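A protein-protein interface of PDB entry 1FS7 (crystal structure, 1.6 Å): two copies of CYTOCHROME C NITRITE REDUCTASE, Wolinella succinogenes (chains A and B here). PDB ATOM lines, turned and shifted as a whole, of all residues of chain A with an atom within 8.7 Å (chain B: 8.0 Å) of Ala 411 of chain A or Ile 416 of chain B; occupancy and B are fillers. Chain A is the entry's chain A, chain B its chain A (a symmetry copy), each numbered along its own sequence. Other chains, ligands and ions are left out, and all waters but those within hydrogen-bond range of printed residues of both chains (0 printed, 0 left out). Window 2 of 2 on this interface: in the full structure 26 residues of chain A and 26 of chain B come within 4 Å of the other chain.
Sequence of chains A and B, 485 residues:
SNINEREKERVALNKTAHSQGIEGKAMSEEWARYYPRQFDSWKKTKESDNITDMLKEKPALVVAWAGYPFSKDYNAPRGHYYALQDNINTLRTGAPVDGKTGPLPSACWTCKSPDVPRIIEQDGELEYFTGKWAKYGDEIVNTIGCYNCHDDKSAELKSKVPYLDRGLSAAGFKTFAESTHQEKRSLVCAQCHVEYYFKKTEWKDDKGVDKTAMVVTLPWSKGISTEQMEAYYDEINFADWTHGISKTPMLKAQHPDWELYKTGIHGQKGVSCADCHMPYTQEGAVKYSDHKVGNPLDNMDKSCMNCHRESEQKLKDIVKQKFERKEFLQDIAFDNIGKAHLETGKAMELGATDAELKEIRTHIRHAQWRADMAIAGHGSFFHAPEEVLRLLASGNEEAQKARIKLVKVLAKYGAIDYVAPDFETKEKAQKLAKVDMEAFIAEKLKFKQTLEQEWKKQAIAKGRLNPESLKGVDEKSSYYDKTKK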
ATOM      1  N   ALA A 347      -7.681 -17.187 -22.991  1.00  0.00           N
ATOM      2  CA  ALA A 347      -6.283 -17.282 -23.407  1.00  0.00           C
ATOM      3  C   ALA A 347      -5.968 -18.703 -23.866  1.00  0.00           C
ATOM      4  O   ALA A 347      -5.260 -18.903 -24.850  1.00  0.00           O
ATOM      5  CB  ALA A 347      -5.362 -16.885 -22.253  1.00  0.00           C
ATOM      6  N   LEU A 350      -7.191 -19.370 -27.272  1.00  0.00           N
ATOM      7  CA  LEU A 350      -6.372 -18.708 -28.282  1.00  0.00           C
ATOM      8  C   LEU A 350      -5.016 -19.390 -28.487  1.00  0.00           C
ATOM      9  O   LEU A 350      -4.291 -19.069 -29.426  1.00  0.00           O
ATOM     10  CB  LEU A 350      -6.164 -17.240 -27.901  1.00  0.00           C
ATOM     11  CG  LEU A 350      -7.448 -16.403 -27.836  1.00  0.00           C
ATOM     12  CD1 LEU A 350      -7.171 -15.057 -27.179  1.00  0.00           C
ATOM     13  CD2 LEU A 350      -8.006 -16.222 -29.240  1.00  0.00           C
ATOM     14  N   ILE A 404      -3.874  -8.627 -14.275  1.00  0.00           N
ATOM     15  CA  ILE A 404      -2.929  -7.712 -14.911  1.00  0.00           C
ATOM     16  C   ILE A 404      -2.034  -8.529 -15.840  1.00  0.00           C
ATOM     17  O   ILE A 404      -1.753  -8.115 -16.967  1.00  0.00           O
ATOM     18  CB  ILE A 404      -2.069  -6.969 -13.854  1.00  0.00           C
ATOM     19  CG1 ILE A 404      -2.945  -5.950 -13.119  1.00  0.00           C
ATOM     20  CG2 ILE A 404      -0.873  -6.274 -14.522  1.00  0.00           C
ATOM     21  CD1 ILE A 404      -2.236  -5.200 -12.011  1.00  0.00           C
ATOM     22  N   LYS A 405      -1.601  -9.695 -15.375  1.00  0.00           N
ATOM     23  CA  LYS A 405      -0.754 -10.560 -16.195  1.00  0.00           C
ATOM     24  C   LYS A 405      -1.552 -11.141 -17.359  1.00  0.00           C
ATOM     25  O   LYS A 405      -1.014 -11.364 -18.444  1.00  0.00           O
ATOM     26  CB  LYS A 405      -0.161 -11.690 -15.346  1.00  0.00           C
ATOM     27  CG  LYS A 405       0.865 -11.193 -14.328  1.00  0.00           C
ATOM     28  CD  LYS A 405       1.448 -12.312 -13.483  1.00  0.00           C
ATOM     29  CE  LYS A 405       2.466 -11.752 -12.495  1.00  0.00           C
ATOM     30  NZ  LYS A 405       3.093 -12.806 -11.643  1.00  0.00           N
ATOM     31  N   LEU A 406      -2.839 -11.388 -17.131  1.00  0.00           N
ATOM     32  CA  LEU A 406      -3.696 -11.936 -18.178  1.00  0.00           C
ATOM     33  C   LEU A 406      -3.903 -10.974 -19.339  1.00  0.00           C
ATOM     34  O   LEU A 406      -4.037 -11.408 -20.481  1.00  0.00           O
ATOM     35  CB  LEU A 406      -5.055 -12.341 -17.605  1.00  0.00           C
ATOM     36  CG  LEU A 406      -5.109 -13.712 -16.935  1.00  0.00           C
ATOM     37  CD1 LEU A 406      -6.339 -13.785 -16.028  1.00  0.00           C
ATOM     38  CD2 LEU A 406      -5.147 -14.812 -17.999  1.00  0.00           C
ATOM     39  N   VAL A 407      -3.944  -9.674 -19.056  1.00  0.00           N
ATOM     40  CA  VAL A 407      -4.116  -8.695 -20.125  1.00  0.00           C
ATOM     41  C   VAL A 407      -2.968  -8.857 -21.114  1.00  0.00           C
ATOM     42  O   VAL A 407      -3.165  -8.792 -22.329  1.00  0.00           O
ATOM     43  CB  VAL A 407      -4.101  -7.239 -19.597  1.00  0.00           C
ATOM     44  CG1 VAL A 407      -4.185  -6.261 -20.771  1.00  0.00           C
ATOM     45  CG2 VAL A 407      -5.264  -7.011 -18.642  1.00  0.00           C
ATOM     46  N   LYS A 408      -1.768  -9.080 -20.586  1.00  0.00           N
ATOM     47  CA  LYS A 408      -0.590  -9.246 -21.428  1.00  0.00           C
ATOM     48  C   LYS A 408      -0.640 -10.530 -22.250  1.00  0.00           C
ATOM     49  O   LYS A 408      -0.259 -10.528 -23.419  1.00  0.00           O
ATOM     50  CB  LYS A 408       0.675  -9.209 -20.568  1.00  0.00           C
ATOM     51  CG  LYS A 408       0.858  -7.883 -19.844  1.00  0.00           C
ATOM     52  CD  LYS A 408       2.131  -7.859 -19.024  1.00  0.00           C
ATOM     53  CE  LYS A 408       2.305  -6.513 -18.341  1.00  0.00           C
ATOM     54  NZ  LYS A 408       1.110  -6.175 -17.522  1.00  0.00           N
ATOM     55  N   VAL A 409      -1.109 -11.623 -21.653  1.00  0.00           N
ATOM     56  CA  VAL A 409      -1.204 -12.881 -22.389  1.00  0.00           C
ATOM     57  C   VAL A 409      -2.272 -12.737 -23.471  1.00  0.00           C
ATOM     58  O   VAL A 409      -2.076 -13.155 -24.613  1.00  0.00           O
ATOM     59  CB  VAL A 409      -1.566 -14.063 -21.460  1.00  0.00           C
ATOM     60  CG1 VAL A 409      -1.730 -15.339 -22.279  1.00  0.00           C
ATOM     61  CG2 VAL A 409      -0.474 -14.250 -20.418  1.00  0.00           C
ATOM     62  N   LEU A 410      -3.406 -12.141 -23.114  1.00  0.00           N
ATOM     63  CA  LEU A 410      -4.473 -11.943 -24.086  1.00  0.00           C
ATOM     64  C   LEU A 410      -3.965 -11.070 -25.236  1.00  0.00           C
ATOM     65  O   LEU A 410      -4.283 -11.316 -26.396  1.00  0.00           O
ATOM     66  CB  LEU A 410      -5.693 -11.288 -23.421  1.00  0.00           C
ATOM     67  CG  LEU A 410      -6.504 -12.173 -22.466  1.00  0.00           C
ATOM     68  CD1 LEU A 410      -7.581 -11.341 -21.776  1.00  0.00           C
ATOM     69  CD2 LEU A 410      -7.139 -13.328 -23.241  1.00  0.00           C
ATOM     70  N   ALA A 411      -3.160 -10.062 -24.914  1.00  0.00           N
ATOM     71  CA  ALA A 411      -2.612  -9.165 -25.930  1.00  0.00           C
ATOM     72  C   ALA A 411      -1.692  -9.917 -26.890  1.00  0.00           C
ATOM     73  O   ALA A 411      -1.742  -9.710 -28.104  1.00  0.00           O
ATOM     74  CB  ALA A 411      -1.848  -8.017 -25.265  1.00  0.00           C
ATOM     75  N   LYS A 412      -0.847 -10.784 -26.347  1.00  0.00           N
ATOM     76  CA  LYS A 412       0.067 -11.555 -27.182  1.00  0.00           C
ATOM     77  C   LYS A 412      -0.703 -12.330 -28.242  1.00  0.00           C
ATOM     78  O   LYS A 412      -0.241 -12.480 -29.380  1.00  0.00           O
ATOM     79  CB  LYS A 412       0.879 -12.540 -26.337  1.00  0.00           C
ATOM     80  CG  LYS A 412       1.708 -13.486 -27.194  1.00  0.00           C
ATOM     81  CD  LYS A 412       2.472 -14.505 -26.379  1.00  0.00           C
ATOM     82  CE  LYS A 412       3.192 -15.471 -27.307  1.00  0.00           C
ATOM     83  NZ  LYS A 412       3.966 -16.495 -26.571  1.00  0.00           N
ATOM     84  N   TYR A 413      -1.879 -12.821 -27.864  1.00  0.00           N
ATOM     85  CA  TYR A 413      -2.711 -13.595 -28.772  1.00  0.00           C
ATOM     86  C   TYR A 413      -3.786 -12.785 -29.496  1.00  0.00           C
ATOM     87  O   TYR A 413      -4.743 -13.342 -30.031  1.00  0.00           O
ATOM     88  CB  TYR A 413      -3.319 -14.776 -28.015  1.00  0.00           C
ATOM     89  CG  TYR A 413      -2.267 -15.805 -27.654  1.00  0.00           C
ATOM     90  CD1 TYR A 413      -1.764 -16.677 -28.620  1.00  0.00           C
ATOM     91  CD2 TYR A 413      -1.715 -15.853 -26.374  1.00  0.00           C
ATOM     92  CE1 TYR A 413      -0.735 -17.567 -28.324  1.00  0.00           C
ATOM     93  CE2 TYR A 413      -0.682 -16.740 -26.064  1.00  0.00           C
ATOM     94  CZ  TYR A 413      -0.195 -17.592 -27.046  1.00  0.00           C
ATOM     95  OH  TYR A 413       0.841 -18.452 -26.765  1.00  0.00           O
ATOM     96  N   GLY A 414      -3.606 -11.467 -29.511  1.00  0.00           N
ATOM     97  CA  GLY A 414      -4.518 -10.576 -30.210  1.00  0.00           C
ATOM     98  C   GLY A 414      -5.896 -10.316 -29.639  1.00  0.00           C
ATOM     99  O   GLY A 414      -6.801  -9.962 -30.388  1.00  0.00           O
ATOM    100  N   ALA A 415      -6.072 -10.459 -28.331  1.00  0.00           N
ATOM    101  CA  ALA A 415      -7.388 -10.226 -27.735  1.00  0.00           C
ATOM    102  C   ALA A 415      -7.308  -9.331 -26.504  1.00  0.00           C
ATOM    103  O   ALA A 415      -7.960  -9.595 -25.496  1.00  0.00           O
ATOM    104  CB  ALA A 415      -8.033 -11.560 -27.368  1.00  0.00           C
ATOM    105  N   ILE A 416      -6.527  -8.261 -26.590  1.00  0.00           N
ATOM    106  CA  ILE A 416      -6.369  -7.367 -25.451  1.00  0.00           C
ATOM    107  C   ILE A 416      -7.682  -6.711 -25.018  1.00  0.00           C
ATOM    108  O   ILE A 416      -7.840  -6.353 -23.849  1.00  0.00           O
ATOM    109  CB  ILE A 416      -5.322  -6.264 -25.740  1.00  0.00           C
ATOM    110  CG1 ILE A 416      -4.833  -5.666 -24.419  1.00  0.00           C
ATOM    111  CG2 ILE A 416      -5.932  -5.162 -26.615  1.00  0.00           C
ATOM    112  CD1 ILE A 416      -3.681  -4.694 -24.568  1.00  0.00           C
ATOM    113  N   ASP A 417      -8.625  -6.564 -25.947  1.00  0.00           N
ATOM    114  CA  ASP A 417      -9.910  -5.937 -25.633  1.00  0.00           C
ATOM    115  C   ASP A 417     -11.007  -6.938 -25.265  1.00  0.00           C
ATOM    116  O   ASP A 417     -12.193  -6.598 -25.258  1.00  0.00           O
ATOM    117  CB  ASP A 417     -10.384  -5.073 -26.807  1.00  0.00           C
ATOM    118  CG  ASP A 417      -9.421  -3.941 -27.123  1.00  0.00           C
ATOM    119  OD1 ASP A 417      -9.085  -3.172 -26.198  1.00  0.00           O
ATOM    120  OD2 ASP A 417      -9.005  -3.820 -28.298  1.00  0.00           O
ATOM    121  N   TYR A 418     -10.614  -8.171 -24.965  1.00  0.00           N
ATOM    122  CA  TYR A 418     -11.578  -9.199 -24.581  1.00  0.00           C
ATOM    123  C   TYR A 418     -12.302  -8.777 -23.308  1.00  0.00           C
ATOM    124  O   TYR A 418     -11.681  -8.256 -22.380  1.00  0.00           O
ATOM    125  CB  TYR A 418     -10.858 -10.527 -24.328  1.00  0.00           C
ATOM    126  CG  TYR A 418     -11.730 -11.613 -23.731  1.00  0.00           C
ATOM    127  CD1 TYR A 418     -12.731 -12.225 -24.482  1.00  0.00           C
ATOM    128  CD2 TYR A 418     -11.538 -12.039 -22.417  1.00  0.00           C
ATOM    129  CE1 TYR A 418     -13.523 -13.241 -23.937  1.00  0.00           C
ATOM    130  CE2 TYR A 418     -12.322 -13.050 -21.863  1.00  0.00           C
ATOM    131  CZ  TYR A 418     -13.310 -13.647 -22.628  1.00  0.00           C
ATOM    132  OH  TYR A 418     -14.077 -14.651 -22.085  1.00  0.00           O
ATOM    133  N   GLU B 343       2.831   4.480 -14.013  1.00  0.00           N
ATOM    134  CA  GLU B 343       2.405   3.920 -15.296  1.00  0.00           C
ATOM    135  C   GLU B 343       1.660   4.974 -16.112  1.00  0.00           C
ATOM    136  O   GLU B 343       1.781   5.026 -17.337  1.00  0.00           O
ATOM    137  CB  GLU B 343       1.528   2.682 -15.058  1.00  0.00           C
ATOM    138  CG  GLU B 343       2.352   1.452 -14.675  1.00  0.00           C
ATOM    139  CD  GLU B 343       1.547   0.363 -13.974  1.00  0.00           C
ATOM    140  OE1 GLU B 343       0.331   0.543 -13.761  1.00  0.00           O
ATOM    141  OE2 GLU B 343       2.142  -0.679 -13.628  1.00  0.00           O
ATOM    142  N   LEU B 350       4.601   8.741 -23.623  1.00  0.00           N
ATOM    143  CA  LEU B 350       4.472   8.088 -24.922  1.00  0.00           C
ATOM    144  C   LEU B 350       3.450   8.776 -25.831  1.00  0.00           C
ATOM    145  O   LEU B 350       3.360   8.464 -27.017  1.00  0.00           O
ATOM    146  CB  LEU B 350       4.092   6.618 -24.729  1.00  0.00           C
ATOM    147  CG  LEU B 350       5.132   5.778 -23.977  1.00  0.00           C
ATOM    148  CD1 LEU B 350       4.543   4.427 -23.590  1.00  0.00           C
ATOM    149  CD2 LEU B 350       6.370   5.606 -24.846  1.00  0.00           C
ATOM    150  N   LEU B 406      -4.583   0.687 -17.599  1.00  0.00           N
ATOM    151  CA  LEU B 406      -3.293   1.241 -17.999  1.00  0.00           C
ATOM    152  C   LEU B 406      -2.481   0.288 -18.864  1.00  0.00           C
ATOM    153  O   LEU B 406      -1.744   0.731 -19.741  1.00  0.00           O
ATOM    154  CB  LEU B 406      -2.474   1.638 -16.771  1.00  0.00           C
ATOM    155  CG  LEU B 406      -2.799   3.004 -16.170  1.00  0.00           C
ATOM    156  CD1 LEU B 406      -2.269   3.066 -14.737  1.00  0.00           C
ATOM    157  CD2 LEU B 406      -2.185   4.113 -17.030  1.00  0.00           C
ATOM    158  N   VAL B 407      -2.599  -1.014 -18.616  1.00  0.00           N
ATOM    159  CA  VAL B 407      -1.866  -1.984 -19.422  1.00  0.00           C
ATOM    160  C   VAL B 407      -2.284  -1.811 -20.878  1.00  0.00           C
ATOM    161  O   VAL B 407      -1.451  -1.868 -21.786  1.00  0.00           O
ATOM    162  CB  VAL B 407      -2.165  -3.445 -19.002  1.00  0.00           C
ATOM    163  CG1 VAL B 407      -1.448  -4.414 -19.945  1.00  0.00           C
ATOM    164  CG2 VAL B 407      -1.716  -3.683 -17.567  1.00  0.00           C
ATOM    165  N   LYS B 408      -3.577  -1.590 -21.094  1.00  0.00           N
ATOM    166  CA  LYS B 408      -4.099  -1.414 -22.442  1.00  0.00           C
ATOM    167  C   LYS B 408      -3.610  -0.124 -23.092  1.00  0.00           C
ATOM    168  O   LYS B 408      -3.287  -0.115 -24.278  1.00  0.00           O
ATOM    169  CB  LYS B 408      -5.629  -1.455 -22.419  1.00  0.00           C
ATOM    170  CG  LYS B 408      -6.176  -2.787 -21.924  1.00  0.00           C
ATOM    171  CD  LYS B 408      -7.691  -2.814 -21.938  1.00  0.00           C
ATOM    172  CE  LYS B 408      -8.208  -4.166 -21.473  1.00  0.00           C
ATOM    173  NZ  LYS B 408      -7.656  -4.514 -20.136  1.00  0.00           N
ATOM    174  N   VAL B 409      -3.548   0.962 -22.327  1.00  0.00           N
ATOM    175  CA  VAL B 409      -3.068   2.226 -22.880  1.00  0.00           C
ATOM    176  C   VAL B 409      -1.580   2.088 -23.199  1.00  0.00           C
ATOM    177  O   VAL B 409      -1.119   2.517 -24.257  1.00  0.00           O
ATOM    178  CB  VAL B 409      -3.278   3.400 -21.895  1.00  0.00           C
ATOM    179  CG1 VAL B 409      -2.694   4.682 -22.478  1.00  0.00           C
ATOM    180  CG2 VAL B 409      -4.764   3.581 -21.621  1.00  0.00           C
ATOM    181  N   LEU B 410      -0.827   1.487 -22.282  1.00  0.00           N
ATOM    182  CA  LEU B 410       0.599   1.295 -22.511  1.00  0.00           C
ATOM    183  C   LEU B 410       0.807   0.432 -23.758  1.00  0.00           C
ATOM    184  O   LEU B 410       1.709   0.687 -24.551  1.00  0.00           O
ATOM    185  CB  LEU B 410       1.254   0.631 -21.291  1.00  0.00           C
ATOM    186  CG  LEU B 410       1.406   1.507 -20.040  1.00  0.00           C
ATOM    187  CD1 LEU B 410       1.930   0.666 -18.879  1.00  0.00           C
ATOM    188  CD2 LEU B 410       2.360   2.666 -20.331  1.00  0.00           C
ATOM    189  N   ALA B 411      -0.040  -0.576 -23.939  1.00  0.00           N
ATOM    190  CA  ALA B 411       0.062  -1.463 -25.097  1.00  0.00           C
ATOM    191  C   ALA B 411      -0.182  -0.702 -26.398  1.00  0.00           C
ATOM    192  O   ALA B 411       0.526  -0.899 -27.387  1.00  0.00           O
ATOM    193  CB  ALA B 411      -0.940  -2.615 -24.969  1.00  0.00           C
ATOM    194  N   LYS B 412      -1.189   0.163 -26.401  1.00  0.00           N
ATOM    195  CA  LYS B 412      -1.496   0.943 -27.594  1.00  0.00           C
ATOM    196  C   LYS B 412      -0.273   1.725 -28.051  1.00  0.00           C
ATOM    197  O   LYS B 412      -0.035   1.885 -29.255  1.00  0.00           O
ATOM    198  CB  LYS B 412      -2.641   1.923 -27.325  1.00  0.00           C
ATOM    199  CG  LYS B 412      -2.867   2.877 -28.489  1.00  0.00           C
ATOM    200  CD  LYS B 412      -3.955   3.892 -28.219  1.00  0.00           C
ATOM    201  CE  LYS B 412      -4.050   4.867 -29.381  1.00  0.00           C
ATOM    202  NZ  LYS B 412      -5.103   5.887 -29.183  1.00  0.00           N
ATOM    203  N   TYR B 413       0.502   2.210 -27.086  1.00  0.00           N
ATOM    204  CA  TYR B 413       1.693   2.989 -27.381  1.00  0.00           C
ATOM    205  C   TYR B 413       2.991   2.182 -27.404  1.00  0.00           C
ATOM    206  O   TYR B 413       4.084   2.741 -27.321  1.00  0.00           O
ATOM    207  CB  TYR B 413       1.783   4.163 -26.406  1.00  0.00           C
ATOM    208  CG  TYR B 413       0.703   5.191 -26.673  1.00  0.00           C
ATOM    209  CD1 TYR B 413       0.811   6.072 -27.749  1.00  0.00           C
ATOM    210  CD2 TYR B 413      -0.461   5.230 -25.905  1.00  0.00           C
ATOM    211  CE1 TYR B 413      -0.214   6.961 -28.059  1.00  0.00           C
ATOM    212  CE2 TYR B 413      -1.497   6.116 -26.207  1.00  0.00           C
ATOM    213  CZ  TYR B 413      -1.367   6.978 -27.287  1.00  0.00           C
ATOM    214  OH  TYR B 413      -2.389   7.838 -27.614  1.00  0.00           O
ATOM    215  N   GLY B 414       2.852   0.865 -27.526  1.00  0.00           N
ATOM    216  CA  GLY B 414       4.000  -0.023 -27.617  1.00  0.00           C
ATOM    217  C   GLY B 414       4.839  -0.291 -26.386  1.00  0.00           C
ATOM    218  O   GLY B 414       6.008  -0.641 -26.518  1.00  0.00           O
ATOM    219  N   ALA B 415       4.269  -0.159 -25.194  1.00  0.00           N
ATOM    220  CA  ALA B 415       5.042  -0.400 -23.976  1.00  0.00           C
ATOM    221  C   ALA B 415       4.302  -1.305 -22.998  1.00  0.00           C
ATOM    222  O   ALA B 415       4.292  -1.051 -21.795  1.00  0.00           O
ATOM    223  CB  ALA B 415       5.376   0.929 -23.303  1.00  0.00           C
ATOM    224  N   ILE B 416       3.699  -2.372 -23.508  1.00  0.00           N
ATOM    225  CA  ILE B 416       2.944  -3.275 -22.649  1.00  0.00           C
ATOM    226  C   ILE B 416       3.806  -3.938 -21.571  1.00  0.00           C
ATOM    227  O   ILE B 416       3.296  -4.306 -20.510  1.00  0.00           O
ATOM    228  CB  ILE B 416       2.230  -4.373 -23.474  1.00  0.00           C
ATOM    229  CG1 ILE B 416       1.098  -4.980 -22.643  1.00  0.00           C
ATOM    230  CG2 ILE B 416       3.222  -5.470 -23.880  1.00  0.00           C
ATOM    231  CD1 ILE B 416       0.219  -5.948 -23.408  1.00  0.00           C
ATOM    232  N   ASP B 417       5.104  -4.079 -21.832  1.00  0.00           N
ATOM    233  CA  ASP B 417       6.007  -4.712 -20.869  1.00  0.00           C
ATOM    234  C   ASP B 417       6.720  -3.717 -19.951  1.00  0.00           C
ATOM    235  O   ASP B 417       7.708  -4.060 -19.297  1.00  0.00           O
ATOM    236  CB  ASP B 417       7.049  -5.567 -21.597  1.00  0.00           C
ATOM    237  CG  ASP B 417       6.421  -6.695 -22.400  1.00  0.00           C
ATOM    238  OD1 ASP B 417       5.634  -7.470 -21.817  1.00  0.00           O
ATOM    239  OD2 ASP B 417       6.718  -6.805 -23.611  1.00  0.00           O
ATOM    240  N   TYR B 418       6.223  -2.485 -19.906  1.00  0.00           N
ATOM    241  CA  TYR B 418       6.816  -1.462 -19.048  1.00  0.00           C
ATOM    242  C   TYR B 418       6.724  -1.897 -17.590  1.00  0.00           C
ATOM    243  O   TYR B 418       5.697  -2.424 -17.159  1.00  0.00           O
ATOM    244  CB  TYR B 418       6.072  -0.135 -19.221  1.00  0.00           C
ATOM    245  CG  TYR B 418       6.471   0.944 -18.235  1.00  0.00           C
ATOM    246  CD1 TYR B 418       7.718   1.559 -18.308  1.00  0.00           C
ATOM    247  CD2 TYR B 418       5.588   1.360 -17.238  1.00  0.00           C
ATOM    248  CE1 TYR B 418       8.079   2.569 -17.409  1.00  0.00           C
ATOM    249  CE2 TYR B 418       5.937   2.365 -16.336  1.00  0.00           C
ATOM    250  CZ  TYR B 418       7.181   2.965 -16.429  1.00  0.00           C
ATOM    251  OH  TYR B 418       7.522   3.963 -15.546  1.00  0.00           O
ATOM    252  N   VAL B 419       7.799  -1.673 -16.840  1.00  0.00           N
ATOM    253  CA  VAL B 419       7.847  -2.019 -15.420  1.00  0.00           C
ATOM    254  C   VAL B 419       8.064  -0.731 -14.633  1.00  0.00           C
ATOM    255  O   VAL B 419       9.131  -0.126 -14.711  1.00  0.00           O
ATOM    256  CB  VAL B 419       9.020  -2.983 -15.105  1.00  0.00           C
ATOM    257  CG1 VAL B 419       9.031  -3.321 -13.616  1.00  0.00           C
ATOM    258  CG2 VAL B 419       8.900  -4.251 -15.941  1.00  0.00           C
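Val 407 of chain A touches Val 407 of chain B (CG1 to CG1, 3.4 Å). Lys 408 of chain B touches Val 407 of chain A. NZ of Lys 408 of chain A touches CG2 of Val 407 of chain B, 3.8 Å away. Ile 416 of chain B touches Lys 408 of chain A (O to CE, 3.2 Å). Ala 411 of chain A touches Ile 416 of chain B. Ile 416 of chain A touches Lys 408 of chain B. Ala 411 of chain B touches Ile 416 of chain A.
Of chain B, only Ile 416 comes within 4 Å of Ala 411 of chain A. Printed residues of chain A within 4 Å of Lys 408 of chain B: Val 407 and Ile 416. Of the printed residues of chain A, Val 407 of chain B touches Val 407 (3.4 Å) and Lys 408 (3.8 Å). Printed residues of chain B within 4 Å of Lys 408 of chain A: Val 407 and Ile 416. Ala 415 of chain A touches none of the printed residues of chain B. Leu 406 of chain B touches none of the printed residues of chain A.
Val 407 of chain A touches its own counterpart, Val 407 of chain B. Val 407 of chain A touches Lys 408 of chain B, and with the chains exchanged Lys 408 of chain A touches Val 407 of chain B. Lys 408 of chain A touches Ile 416 of chain B, and with the chains exchanged Ile 416 of chain A touches Lys 408 of chain B. Ala 411 of chain A touches Ile 416 of chain B, and with the chains exchanged Ile 416 of chain A touches Ala 411 of chain B. Positions printed for both chains: 350, 406, 407, 408, 409, 410, 411, 412, 413, 414, 415, 416, 417 and 418.
Printed residues of chain A that touch a printed residue of chain B: Val 407, Lys 408, Ala 411 and Ile 416. Hydrophobic or aromatic side chains of chain A within 4 Å of the printed part of chain B: Val 407, Ala 411 and Ile 416. Printed residues of chain B that touch a printed residue of chain A: Val 407, Lys 408, Ala 411 and Ile 416. Hydrophobic or aromatic side chains of chain B that line the printed part of chain A: Val 407, Ala 411 and Ile 416. Along chain B the printed residues that touch a printed residue of chain A span positions 407 to 416. Among the printed residues, 7 pairs touch across the chains. Among the printed residues, no Asp or Glu carboxylate lies within 4 Å of a Lys or Arg side-chain nitrogen of the other chain.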
